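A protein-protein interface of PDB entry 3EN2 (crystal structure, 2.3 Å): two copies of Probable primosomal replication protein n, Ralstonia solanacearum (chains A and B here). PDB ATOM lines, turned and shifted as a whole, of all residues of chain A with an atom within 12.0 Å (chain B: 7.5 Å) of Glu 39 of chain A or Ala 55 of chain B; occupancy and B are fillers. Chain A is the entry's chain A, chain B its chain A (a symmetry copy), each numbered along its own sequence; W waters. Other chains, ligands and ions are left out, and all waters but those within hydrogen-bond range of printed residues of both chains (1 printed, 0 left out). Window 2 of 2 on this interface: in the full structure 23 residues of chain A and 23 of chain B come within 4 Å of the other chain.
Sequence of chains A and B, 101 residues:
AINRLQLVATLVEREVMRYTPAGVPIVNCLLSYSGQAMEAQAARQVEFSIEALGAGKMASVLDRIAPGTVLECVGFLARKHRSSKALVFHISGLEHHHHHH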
ATOM      1  N   TYR A  33       9.123 -38.947  -2.563  1.00  0.00           N
ATOM      2  CA  TYR A  33       8.756 -37.565  -2.284  1.00  0.00           C
ATOM      3  C   TYR A  33       8.266 -36.811  -3.521  1.00  0.00           C
ATOM      4  O   TYR A  33       8.821 -36.960  -4.603  1.00  0.00           O
ATOM      5  CB  TYR A  33       9.942 -36.807  -1.685  1.00  0.00           C
ATOM      6  CG  TYR A  33       9.657 -35.338  -1.550  1.00  0.00           C
ATOM      7  CD1 TYR A  33       9.986 -34.443  -2.568  1.00  0.00           C
ATOM      8  CD2 TYR A  33       8.973 -34.853  -0.447  1.00  0.00           C
ATOM      9  CE1 TYR A  33       9.627 -33.093  -2.490  1.00  0.00           C
ATOM     10  CE2 TYR A  33       8.607 -33.506  -0.357  1.00  0.00           C
ATOM     11  CZ  TYR A  33       8.933 -32.632  -1.380  1.00  0.00           C
ATOM     12  OH  TYR A  33       8.555 -31.308  -1.289  1.00  0.00           O
ATOM     13  N   GLY A  35       6.667 -32.750  -4.285  1.00  0.00           N
ATOM     14  CA  GLY A  35       6.254 -31.463  -3.752  1.00  0.00           C
ATOM     15  C   GLY A  35       7.045 -30.354  -4.402  1.00  0.00           C
ATOM     16  O   GLY A  35       7.613 -30.540  -5.471  1.00  0.00           O
ATOM     17  N   GLN A  36       7.091 -29.197  -3.759  1.00  0.00           N
ATOM     18  CA  GLN A  36       7.831 -28.075  -4.313  1.00  0.00           C
ATOM     19  C   GLN A  36       8.810 -27.484  -3.312  1.00  0.00           C
ATOM     20  O   GLN A  36       8.649 -27.638  -2.104  1.00  0.00           O
ATOM     21  CB  GLN A  36       6.869 -26.985  -4.787  1.00  0.00           C
ATOM     22  CG  GLN A  36       5.924 -27.422  -5.897  1.00  0.00           C
ATOM     23  CD  GLN A  36       5.325 -26.247  -6.639  1.00  0.00           C
ATOM     24  OE1 GLN A  36       4.772 -25.335  -6.029  1.00  0.00           O
ATOM     25  NE2 GLN A  36       5.432 -26.263  -7.964  1.00  0.00           N
ATOM     26  N   ALA A  37       9.829 -26.813  -3.835  1.00  0.00           N
ATOM     27  CA  ALA A  37      10.844 -26.182  -3.016  1.00  0.00           C
ATOM     28  C   ALA A  37      10.976 -24.719  -3.429  1.00  0.00           C
ATOM     29  O   ALA A  37      10.231 -24.241  -4.280  1.00  0.00           O
ATOM     30  CB  ALA A  37      12.172 -26.897  -3.200  1.00  0.00           C
ATOM     31  N   MET A  38      11.920 -24.010  -2.816  1.00  0.00           N
ATOM     32  CA  MET A  38      12.160 -22.603  -3.129  1.00  0.00           C
ATOM     33  C   MET A  38      13.645 -22.345  -3.355  1.00  0.00           C
ATOM     34  O   MET A  38      14.427 -22.285  -2.404  1.00  0.00           O
ATOM     35  CB  MET A  38      11.638 -21.713  -1.998  1.00  0.00           C
ATOM     36  CG  MET A  38      10.157 -21.379  -2.106  1.00  0.00           C
ATOM     37  SD  MET A  38       9.758 -20.255  -3.648  1.00  0.00           S
ATOM     38  CE  MET A  38       9.688 -18.529  -2.766  1.00  0.00           C
ATOM     39  N   GLU A  39      14.029 -22.191  -4.618  1.00  0.00           N
ATOM     40  CA  GLU A  39      15.428 -21.946  -4.957  1.00  0.00           C
ATOM     41  C   GLU A  39      15.594 -20.772  -5.929  1.00  0.00           C
ATOM     42  O   GLU A  39      14.964 -20.717  -6.981  1.00  0.00           O
ATOM     43  CB  GLU A  39      16.037 -23.213  -5.554  1.00  0.00           C
ATOM     44  CG  GLU A  39      17.538 -23.151  -5.773  1.00  0.00           C
ATOM     45  CD  GLU A  39      18.117 -24.483  -6.207  1.00  0.00           C
ATOM     46  OE1 GLU A  39      17.709 -24.991  -7.273  1.00  0.00           O
ATOM     47  OE2 GLU A  39      18.972 -25.025  -5.478  1.00  0.00           O
ATOM     48  N   ALA A  42      12.838 -18.901  -7.257  1.00  0.00           N
ATOM     49  CA  ALA A  42      11.837 -19.465  -8.156  1.00  0.00           C
ATOM     50  C   ALA A  42      11.384 -20.855  -7.705  1.00  0.00           C
ATOM     51  O   ALA A  42      12.206 -21.758  -7.547  1.00  0.00           O
ATOM     52  CB  ALA A  42      12.389 -19.539  -9.577  1.00  0.00           C
ATOM     53  N   ALA A  43      10.077 -21.025  -7.511  1.00  0.00           N
ATOM     54  CA  ALA A  43       9.524 -22.310  -7.096  1.00  0.00           C
ATOM     55  C   ALA A  43      10.010 -23.404  -8.039  1.00  0.00           C
ATOM     56  O   ALA A  43      10.165 -23.179  -9.241  1.00  0.00           O
ATOM     57  CB  ALA A  43       8.008 -22.256  -7.088  1.00  0.00           C
ATOM     58  N   ARG A  44      10.226 -24.592  -7.484  1.00  0.00           N
ATOM     59  CA  ARG A  44      10.735 -25.726  -8.241  1.00  0.00           C
ATOM     60  C   ARG A  44      10.046 -27.024  -7.831  1.00  0.00           C
ATOM     61  O   ARG A  44      10.033 -27.382  -6.651  1.00  0.00           O
ATOM     62  CB  ARG A  44      12.237 -25.837  -7.984  1.00  0.00           C
ATOM     63  CG  ARG A  44      12.983 -26.960  -8.678  1.00  0.00           C
ATOM     64  CD  ARG A  44      14.405 -26.983  -8.132  1.00  0.00           C
ATOM     65  NE  ARG A  44      15.334 -27.849  -8.857  1.00  0.00           N
ATOM     66  CZ  ARG A  44      15.238 -29.173  -8.932  1.00  0.00           C
ATOM     67  NH1 ARG A  44      14.240 -29.810  -8.331  1.00  0.00           N
ATOM     68  NH2 ARG A  44      16.164 -29.863  -9.586  1.00  0.00           N
ATOM     69  N   GLN A  45       9.466 -27.725  -8.800  1.00  0.00           N
ATOM     70  CA  GLN A  45       8.809 -28.994  -8.510  1.00  0.00           C
ATOM     71  C   GLN A  45       9.939 -29.974  -8.219  1.00  0.00           C
ATOM     72  O   GLN A  45      10.943 -30.002  -8.930  1.00  0.00           O
ATOM     73  CB  GLN A  45       8.003 -29.471  -9.719  1.00  0.00           C
ATOM     74  CG  GLN A  45       7.075 -30.658  -9.448  1.00  0.00           C
ATOM     75  CD  GLN A  45       5.943 -30.315  -8.493  1.00  0.00           C
ATOM     76  OE1 GLN A  45       5.389 -29.215  -8.546  1.00  0.00           O
ATOM     77  NE2 GLN A  45       5.580 -31.262  -7.624  1.00  0.00           N
ATOM     78  N   VAL A  46       9.782 -30.767  -7.168  1.00  0.00           N
ATOM     79  CA  VAL A  46      10.809 -31.731  -6.793  1.00  0.00           C
ATOM     80  C   VAL A  46      10.229 -33.124  -6.595  1.00  0.00           C
ATOM     81  O   VAL A  46       9.229 -33.303  -5.894  1.00  0.00           O
ATOM     82  CB  VAL A  46      11.515 -31.310  -5.482  1.00  0.00           C
ATOM     83  CG1 VAL A  46      12.485 -32.396  -5.032  1.00  0.00           C
ATOM     84  CG2 VAL A  46      12.247 -29.991  -5.688  1.00  0.00           C
ATOM     85  N   GLU A  47      10.856 -34.110  -7.222  1.00  0.00           N
ATOM     86  CA  GLU A  47      10.411 -35.485  -7.079  1.00  0.00           C
ATOM     87  C   GLU A  47      11.619 -36.401  -6.984  1.00  0.00           C
ATOM     88  O   GLU A  47      12.565 -36.283  -7.762  1.00  0.00           O
ATOM     89  CB  GLU A  47       9.552 -35.914  -8.268  1.00  0.00           C
ATOM     90  CG  GLU A  47       8.905 -37.288  -8.080  1.00  0.00           C
ATOM     91  CD  GLU A  47       8.315 -37.856  -9.364  1.00  0.00           C
ATOM     92  OE1 GLU A  47       7.665 -37.091 -10.116  1.00  0.00           O
ATOM     93  OE2 GLU A  47       8.490 -39.073  -9.611  1.00  0.00           O
ATOM     94  N   THR B  20      22.859 -22.373 -15.931  1.00  0.00           N
ATOM     95  CA  THR B  20      21.748 -23.074 -16.548  1.00  0.00           C
ATOM     96  C   THR B  20      21.477 -22.283 -17.831  1.00  0.00           C
ATOM     97  O   THR B  20      21.985 -21.172 -17.995  1.00  0.00           O
ATOM     98  CB  THR B  20      20.486 -23.033 -15.662  1.00  0.00           C
ATOM     99  OG1 THR B  20      19.980 -21.697 -15.607  1.00  0.00           O
ATOM    100  CG2 THR B  20      20.806 -23.500 -14.253  1.00  0.00           C
ATOM    101  N   VAL B  24      21.288 -18.824 -14.748  1.00  0.00           N
ATOM    102  CA  VAL B  24      21.338 -18.936 -13.295  1.00  0.00           C
ATOM    103  C   VAL B  24      22.631 -19.664 -12.926  1.00  0.00           C
ATOM    104  O   VAL B  24      22.855 -20.807 -13.335  1.00  0.00           O
ATOM    105  CB  VAL B  24      20.135 -19.734 -12.742  1.00  0.00           C
ATOM    106  CG1 VAL B  24      20.238 -19.857 -11.221  1.00  0.00           C
ATOM    107  CG2 VAL B  24      18.842 -19.034 -13.128  1.00  0.00           C
ATOM    108  N   PRO B  25      23.510 -19.000 -12.161  1.00  0.00           N
ATOM    109  CA  PRO B  25      24.782 -19.597 -11.747  1.00  0.00           C
ATOM    110  C   PRO B  25      24.616 -20.780 -10.802  1.00  0.00           C
ATOM    111  O   PRO B  25      23.712 -20.803  -9.971  1.00  0.00           O
ATOM    112  CB  PRO B  25      25.508 -18.431 -11.086  1.00  0.00           C
ATOM    113  CG  PRO B  25      24.393 -17.659 -10.465  1.00  0.00           C
ATOM    114  CD  PRO B  25      23.348 -17.657 -11.571  1.00  0.00           C
ATOM    115  N   ILE B  26      25.500 -21.758 -10.932  1.00  0.00           N
ATOM    116  CA  ILE B  26      25.439 -22.926 -10.072  1.00  0.00           C
ATOM    117  C   ILE B  26      26.815 -23.412  -9.682  1.00  0.00           C
ATOM    118  O   ILE B  26      27.703 -23.542 -10.518  1.00  0.00           O
ATOM    119  CB  ILE B  26      24.696 -24.097 -10.750  1.00  0.00           C
ATOM    120  CG1 ILE B  26      23.206 -23.757 -10.894  1.00  0.00           C
ATOM    121  CG2 ILE B  26      24.892 -25.373  -9.937  1.00  0.00           C
ATOM    122  CD1 ILE B  26      22.382 -24.854 -11.523  1.00  0.00           C
ATOM    123  N   VAL B  27      26.991 -23.675  -8.397  1.00  0.00           N
ATOM    124  CA  VAL B  27      28.257 -24.182  -7.910  1.00  0.00           C
ATOM    125  C   VAL B  27      27.988 -25.510  -7.229  1.00  0.00           C
ATOM    126  O   VAL B  27      27.256 -25.578  -6.241  1.00  0.00           O
ATOM    127  CB  VAL B  27      28.914 -23.220  -6.892  1.00  0.00           C
ATOM    128  CG1 VAL B  27      30.080 -23.911  -6.203  1.00  0.00           C
ATOM    129  CG2 VAL B  27      29.400 -21.978  -7.598  1.00  0.00           C
ATOM    130  N   LEU B  53      24.898 -28.278  -3.905  1.00  0.00           N
ATOM    131  CA  LEU B  53      25.042 -27.207  -4.879  1.00  0.00           C
ATOM    132  C   LEU B  53      24.289 -25.969  -4.438  1.00  0.00           C
ATOM    133  O   LEU B  53      23.325 -26.053  -3.678  1.00  0.00           O
ATOM    134  CB  LEU B  53      24.558 -27.660  -6.264  1.00  0.00           C
ATOM    135  CG  LEU B  53      23.066 -27.870  -6.497  1.00  0.00           C
ATOM    136  CD1 LEU B  53      22.352 -26.527  -6.537  1.00  0.00           C
ATOM    137  CD2 LEU B  53      22.855 -28.598  -7.810  1.00  0.00           C
ATOM    138  N   GLY B  54      24.756 -24.821  -4.913  1.00  0.00           N
ATOM    139  CA  GLY B  54      24.124 -23.559  -4.599  1.00  0.00           C
ATOM    140  C   GLY B  54      23.738 -22.923  -5.918  1.00  0.00           C
ATOM    141  O   GLY B  54      24.513 -22.956  -6.873  1.00  0.00           O
ATOM    142  N   ALA B  55      22.538 -22.362  -5.986  1.00  0.00           N
ATOM    143  CA  ALA B  55      22.076 -21.731  -7.218  1.00  0.00           C
ATOM    144  C   ALA B  55      21.782 -20.258  -6.977  1.00  0.00           C
ATOM    145  O   ALA B  55      21.326 -19.879  -5.903  1.00  0.00           O
ATOM    146  CB  ALA B  55      20.832 -22.435  -7.723  1.00  0.00           C
ATOM    147  N   GLY B  56      22.036 -19.426  -7.982  1.00  0.00           N
ATOM    148  CA  GLY B  56      21.781 -18.005  -7.830  1.00  0.00           C
ATOM    149  C   GLY B  56      22.729 -17.395  -6.819  1.00  0.00           C
ATOM    150  O   GLY B  56      23.928 -17.650  -6.862  1.00  0.00           O
ATOM    151  N   LYS B  57      22.203 -16.594  -5.903  1.00  0.00           N
ATOM    152  CA  LYS B  57      23.046 -15.956  -4.894  1.00  0.00           C
ATOM    153  C   LYS B  57      23.872 -16.982  -4.113  1.00  0.00           C
ATOM    154  O   LYS B  57      25.024 -16.721  -3.760  1.00  0.00           O
ATOM    155  CB  LYS B  57      22.185 -15.130  -3.937  1.00  0.00           C
ATOM    156  CG  LYS B  57      22.934 -14.540  -2.745  1.00  0.00           C
ATOM    157  CD  LYS B  57      24.071 -13.604  -3.143  1.00  0.00           C
ATOM    158  CE  LYS B  57      24.721 -12.988  -1.894  1.00  0.00           C
ATOM    159  NZ  LYS B  57      26.058 -12.346  -2.148  1.00  0.00           N
ATOM    160  N   MET B  58      23.288 -18.152  -3.860  1.00  0.00           N
ATOM    161  CA  MET B  58      23.982 -19.207  -3.131  1.00  0.00           C
ATOM    162  C   MET B  58      25.193 -19.715  -3.904  1.00  0.00           C
ATOM    163  O   MET B  58      26.169 -20.175  -3.312  1.00  0.00           O
ATOM    164  CB  MET B  58      23.039 -20.375  -2.830  1.00  0.00           C
ATOM    165  CG  MET B  58      22.273 -20.243  -1.524  1.00  0.00           C
ATOM    166  SD  MET B  58      23.387 -19.986   0.052  1.00  0.00           S
ATOM    167  CE  MET B  58      24.854 -21.094  -0.444  1.00  0.00           C
ATOM    168  N   ALA B  59      25.132 -19.635  -5.225  1.00  0.00           N
ATOM    169  CA  ALA B  59      26.253 -20.075  -6.042  1.00  0.00           C
ATOM    170  C   ALA B  59      27.398 -19.085  -5.834  1.00  0.00           C
ATOM    171  O   ALA B  59      28.552 -19.483  -5.714  1.00  0.00           O
ATOM    172  CB  ALA B  59      25.851 -20.117  -7.505  1.00  0.00           C
ATOM    173  N   SER B  60      27.066 -17.795  -5.784  1.00  0.00           N
ATOM    174  CA  SER B  60      28.062 -16.749  -5.565  1.00  0.00           C
ATOM    175  C   SER B  60      28.682 -16.909  -4.172  1.00  0.00           C
ATOM    176  O   SER B  60      29.892 -16.786  -4.008  1.00  0.00           O
ATOM    177  CB  SER B  60      27.425 -15.354  -5.669  1.00  0.00           C
ATOM    178  OG  SER B  60      26.896 -15.105  -6.962  1.00  0.00           O
ATOM    179  N   LEU B  62      28.937 -19.648  -2.210  1.00  0.00           N
ATOM    180  CA  LEU B  62      29.809 -20.819  -2.136  1.00  0.00           C
ATOM    181  C   LEU B  62      31.106 -20.577  -2.899  1.00  0.00           C
ATOM    182  O   LEU B  62      32.170 -21.048  -2.500  1.00  0.00           O
ATOM    183  CB  LEU B  62      29.105 -22.050  -2.726  1.00  0.00           C
ATOM    184  CG  LEU B  62      27.976 -22.687  -1.916  1.00  0.00           C
ATOM    185  CD1 LEU B  62      27.306 -23.769  -2.745  1.00  0.00           C
ATOM    186  CD2 LEU B  62      28.538 -23.271  -0.619  1.00  0.00           C
ATOM    187  N   PHE B  76      17.119 -28.394   0.763  1.00  0.00           N
ATOM    188  CA  PHE B  76      16.264 -29.514   0.406  1.00  0.00           C
ATOM    189  C   PHE B  76      17.008 -30.513  -0.475  1.00  0.00           C
ATOM    190  O   PHE B  76      18.012 -30.180  -1.091  1.00  0.00           O
ATOM    191  CB  PHE B  76      15.014 -28.997  -0.315  1.00  0.00           C
ATOM    192  CG  PHE B  76      15.301 -28.234  -1.595  1.00  0.00           C
ATOM    193  CD1 PHE B  76      15.241 -28.871  -2.834  1.00  0.00           C
ATOM    194  CD2 PHE B  76      15.609 -26.880  -1.563  1.00  0.00           C
ATOM    195  CE1 PHE B  76      15.481 -28.168  -4.032  1.00  0.00           C
ATOM    196  CE2 PHE B  76      15.853 -26.163  -2.751  1.00  0.00           C
ATOM    197  CZ  PHE B  76      15.785 -26.816  -3.979  1.00  0.00           C
ATOM    198  N   ALA B  78      17.147 -33.278  -3.709  1.00  0.00           N
ATOM    199  CA  ALA B  78      16.565 -33.395  -5.036  1.00  0.00           C
ATOM    200  C   ALA B  78      17.336 -34.415  -5.866  1.00  0.00           C
ATOM    201  O   ALA B  78      18.405 -34.873  -5.469  1.00  0.00           O
ATOM    202  CB  ALA B  78      16.562 -32.043  -5.730  1.00  0.00           C
ATOM    203  N   PHE B  89      22.189 -32.244  -2.397  1.00  0.00           N
ATOM    204  CA  PHE B  89      21.699 -31.346  -1.360  1.00  0.00           C
ATOM    205  C   PHE B  89      21.667 -29.904  -1.874  1.00  0.00           C
ATOM    206  O   PHE B  89      22.713 -29.292  -2.097  1.00  0.00           O
ATOM    207  CB  PHE B  89      22.620 -31.471  -0.130  1.00  0.00           C
ATOM    208  CG  PHE B  89      22.302 -30.513   1.000  1.00  0.00           C
ATOM    209  CD1 PHE B  89      21.012 -30.042   1.215  1.00  0.00           C
ATOM    210  CD2 PHE B  89      23.301 -30.139   1.897  1.00  0.00           C
ATOM    211  CE1 PHE B  89      20.725 -29.212   2.311  1.00  0.00           C
ATOM    212  CE2 PHE B  89      23.024 -29.314   2.990  1.00  0.00           C
ATOM    213  CZ  PHE B  89      21.732 -28.852   3.196  1.00  0.00           C
ATOM    214  N   HIS B  90      20.468 -29.370  -2.083  1.00  0.00           N
ATOM    215  CA  HIS B  90      20.330 -27.994  -2.551  1.00  0.00           C
ATOM    216  C   HIS B  90      20.350 -27.076  -1.329  1.00  0.00           C
ATOM    217  O   HIS B  90      19.450 -27.132  -0.484  1.00  0.00           O
ATOM    218  CB  HIS B  90      19.010 -27.816  -3.309  1.00  0.00           C
ATOM    219  CG  HIS B  90      19.007 -28.413  -4.682  1.00  0.00           C
ATOM    220  ND1 HIS B  90      18.717 -27.672  -5.807  1.00  0.00           N
ATOM    221  CD2 HIS B  90      19.243 -29.674  -5.114  1.00  0.00           C
ATOM    222  CE1 HIS B  90      18.773 -28.451  -6.873  1.00  0.00           C
ATOM    223  NE2 HIS B  90      19.091 -29.670  -6.481  1.00  0.00           N
ATOM    224  N   ILE B  91      21.383 -26.244  -1.230  1.00  0.00           N
ATOM    225  CA  ILE B  91      21.528 -25.324  -0.110  1.00  0.00           C
ATOM    226  C   ILE B  91      20.782 -24.039  -0.400  1.00  0.00           C
ATOM    227  O   ILE B  91      21.070 -23.360  -1.392  1.00  0.00           O
ATOM    228  CB  ILE B  91      23.005 -24.970   0.131  1.00  0.00           C
ATOM    229  CG1 ILE B  91      23.816 -26.248   0.322  1.00  0.00           C
ATOM    230  CG2 ILE B  91      23.134 -24.082   1.365  1.00  0.00           C
ATOM    231  CD1 ILE B  91      25.290 -26.025   0.343  1.00  0.00           C
ATOM    232  N   SER B  92      19.833 -23.700   0.462  1.00  0.00           N
ATOM    233  CA  SER B  92      19.066 -22.481   0.274  1.00  0.00           C
ATOM    234  C   SER B  92      19.448 -21.422   1.314  1.00  0.00           C
ATOM    235  O   SER B  92      19.127 -20.245   1.158  1.00  0.00           O
ATOM    236  CB  SER B  92      17.573 -22.786   0.353  1.00  0.00           C
ATOM    237  OG  SER B  92      17.254 -23.370   1.593  1.00  0.00           O
HETATM  238  O   HOH W   1      20.710 -23.069  -3.943  1.00  0.00           O
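Glu 39 of chain A touches four residues of chain B. Of chain A, only Glu 39 comes within 4 Å of Ala 55 of chain B. Pro 25 of chain B touches none of the printed residues of chain A. No residue of chain A comes within 4 Å of Ile 26 of chain B. No residue of chain A comes within 4 Å of Val 27 of chain B. Leu 53 of chain B touches just one residue of chain A: Glu 39. No residue of chain A comes within 4 Å of Gly 54 of chain B. No residue of chain A comes within 4 Å of Met 58 of chain B. Of chain A, only Ala 37 (3.6 Å) and Glu 39 (3.9 Å) come within 4 Å of Phe 76 of chain B. No residue of chain A comes within 4 Å of Ile 91 of chain B. No residue of chain A comes within 4 Å of Ser 92 of chain B. Of the printed residues of chain B, Ala 37 of chain A touches Phe 76 (3.6 Å). Of the printed residues of chain A, His 90 of chain B touches Glu 39. Glu 47 of chain A touches none of the printed residues of chain B. Val 46 of chain A touches none of the printed residues of chain B. The nearest residue of chain B that does not touch Glu 39 of chain A is Ile 91 of chain B (4.9 Å). The nearest residue of chain A that does not touch Ala 55 of chain B is Arg 44 of chain A (7.8 Å). The nearest printed residue of chain B that does not touch Ala 37 of chain A is His 90 of chain B (6.9 Å).
Among the printed residues, pairs that only touch across the chains: Ala 37 of chain A with Phe 76 of chain B (3.6 Å), Glu 39 of chain A with Leu 53 of chain B (3.8 Å), Glu 39 of chain A with Ala 55 of chain B (3.7 Å) and Glu 39 of chain A with Phe 76 of chain B (3.9 Å).
Water W1 lies within hydrogen-bond range of O of Ile 91 of chain B (2.6 Å), N of Ala 55 of chain B (2.8 Å) and OE2 of Glu 39 of chain A (3.0 Å).
Hydrophobic or aromatic side chains of chain B that line the printed part of chain A: Leu 53, Ala 55, Phe 76 and His 90. Of the 12 printed residues of chain A, 2 touch a printed residue of chain B. Printed residues of chain A that touch a printed residue of chain B: Ala 37 and Glu 39. Hydrophobic or aromatic side chains of chain A that line the printed part of chain B: Ala 37. Along chain A the printed residues that touch a printed residue of chain B span positions 37 to 39. Among the printed residues, 5 pairs touch across the chains.
The side-chain carboxylate (OE2) of Glu 39 of chain A lies within hydrogen-bond range of a ring nitrogen (ND1) of His 90 of chain B, at 2.7 Å.
O of Arg 44 of chain A sits at hydrogen-bond distance from N of Ala 37 of chain A. O of Phe 89 of chain B sits at hydrogen-bond distance from N of Leu 53 of chain B (3.0 Å). N of Ile 91 of chain B sits at hydrogen-bond distance from O of Leu 53 of chain B, at 3.1 Å. N of His 90 of chain B is in hydrogen-bond range of O of Phe 76 of chain B.
No position is printed for both chains. Of the 5 pairs that touch across the chains among the printed residues, none has its exchanged pair printed and touching as well.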
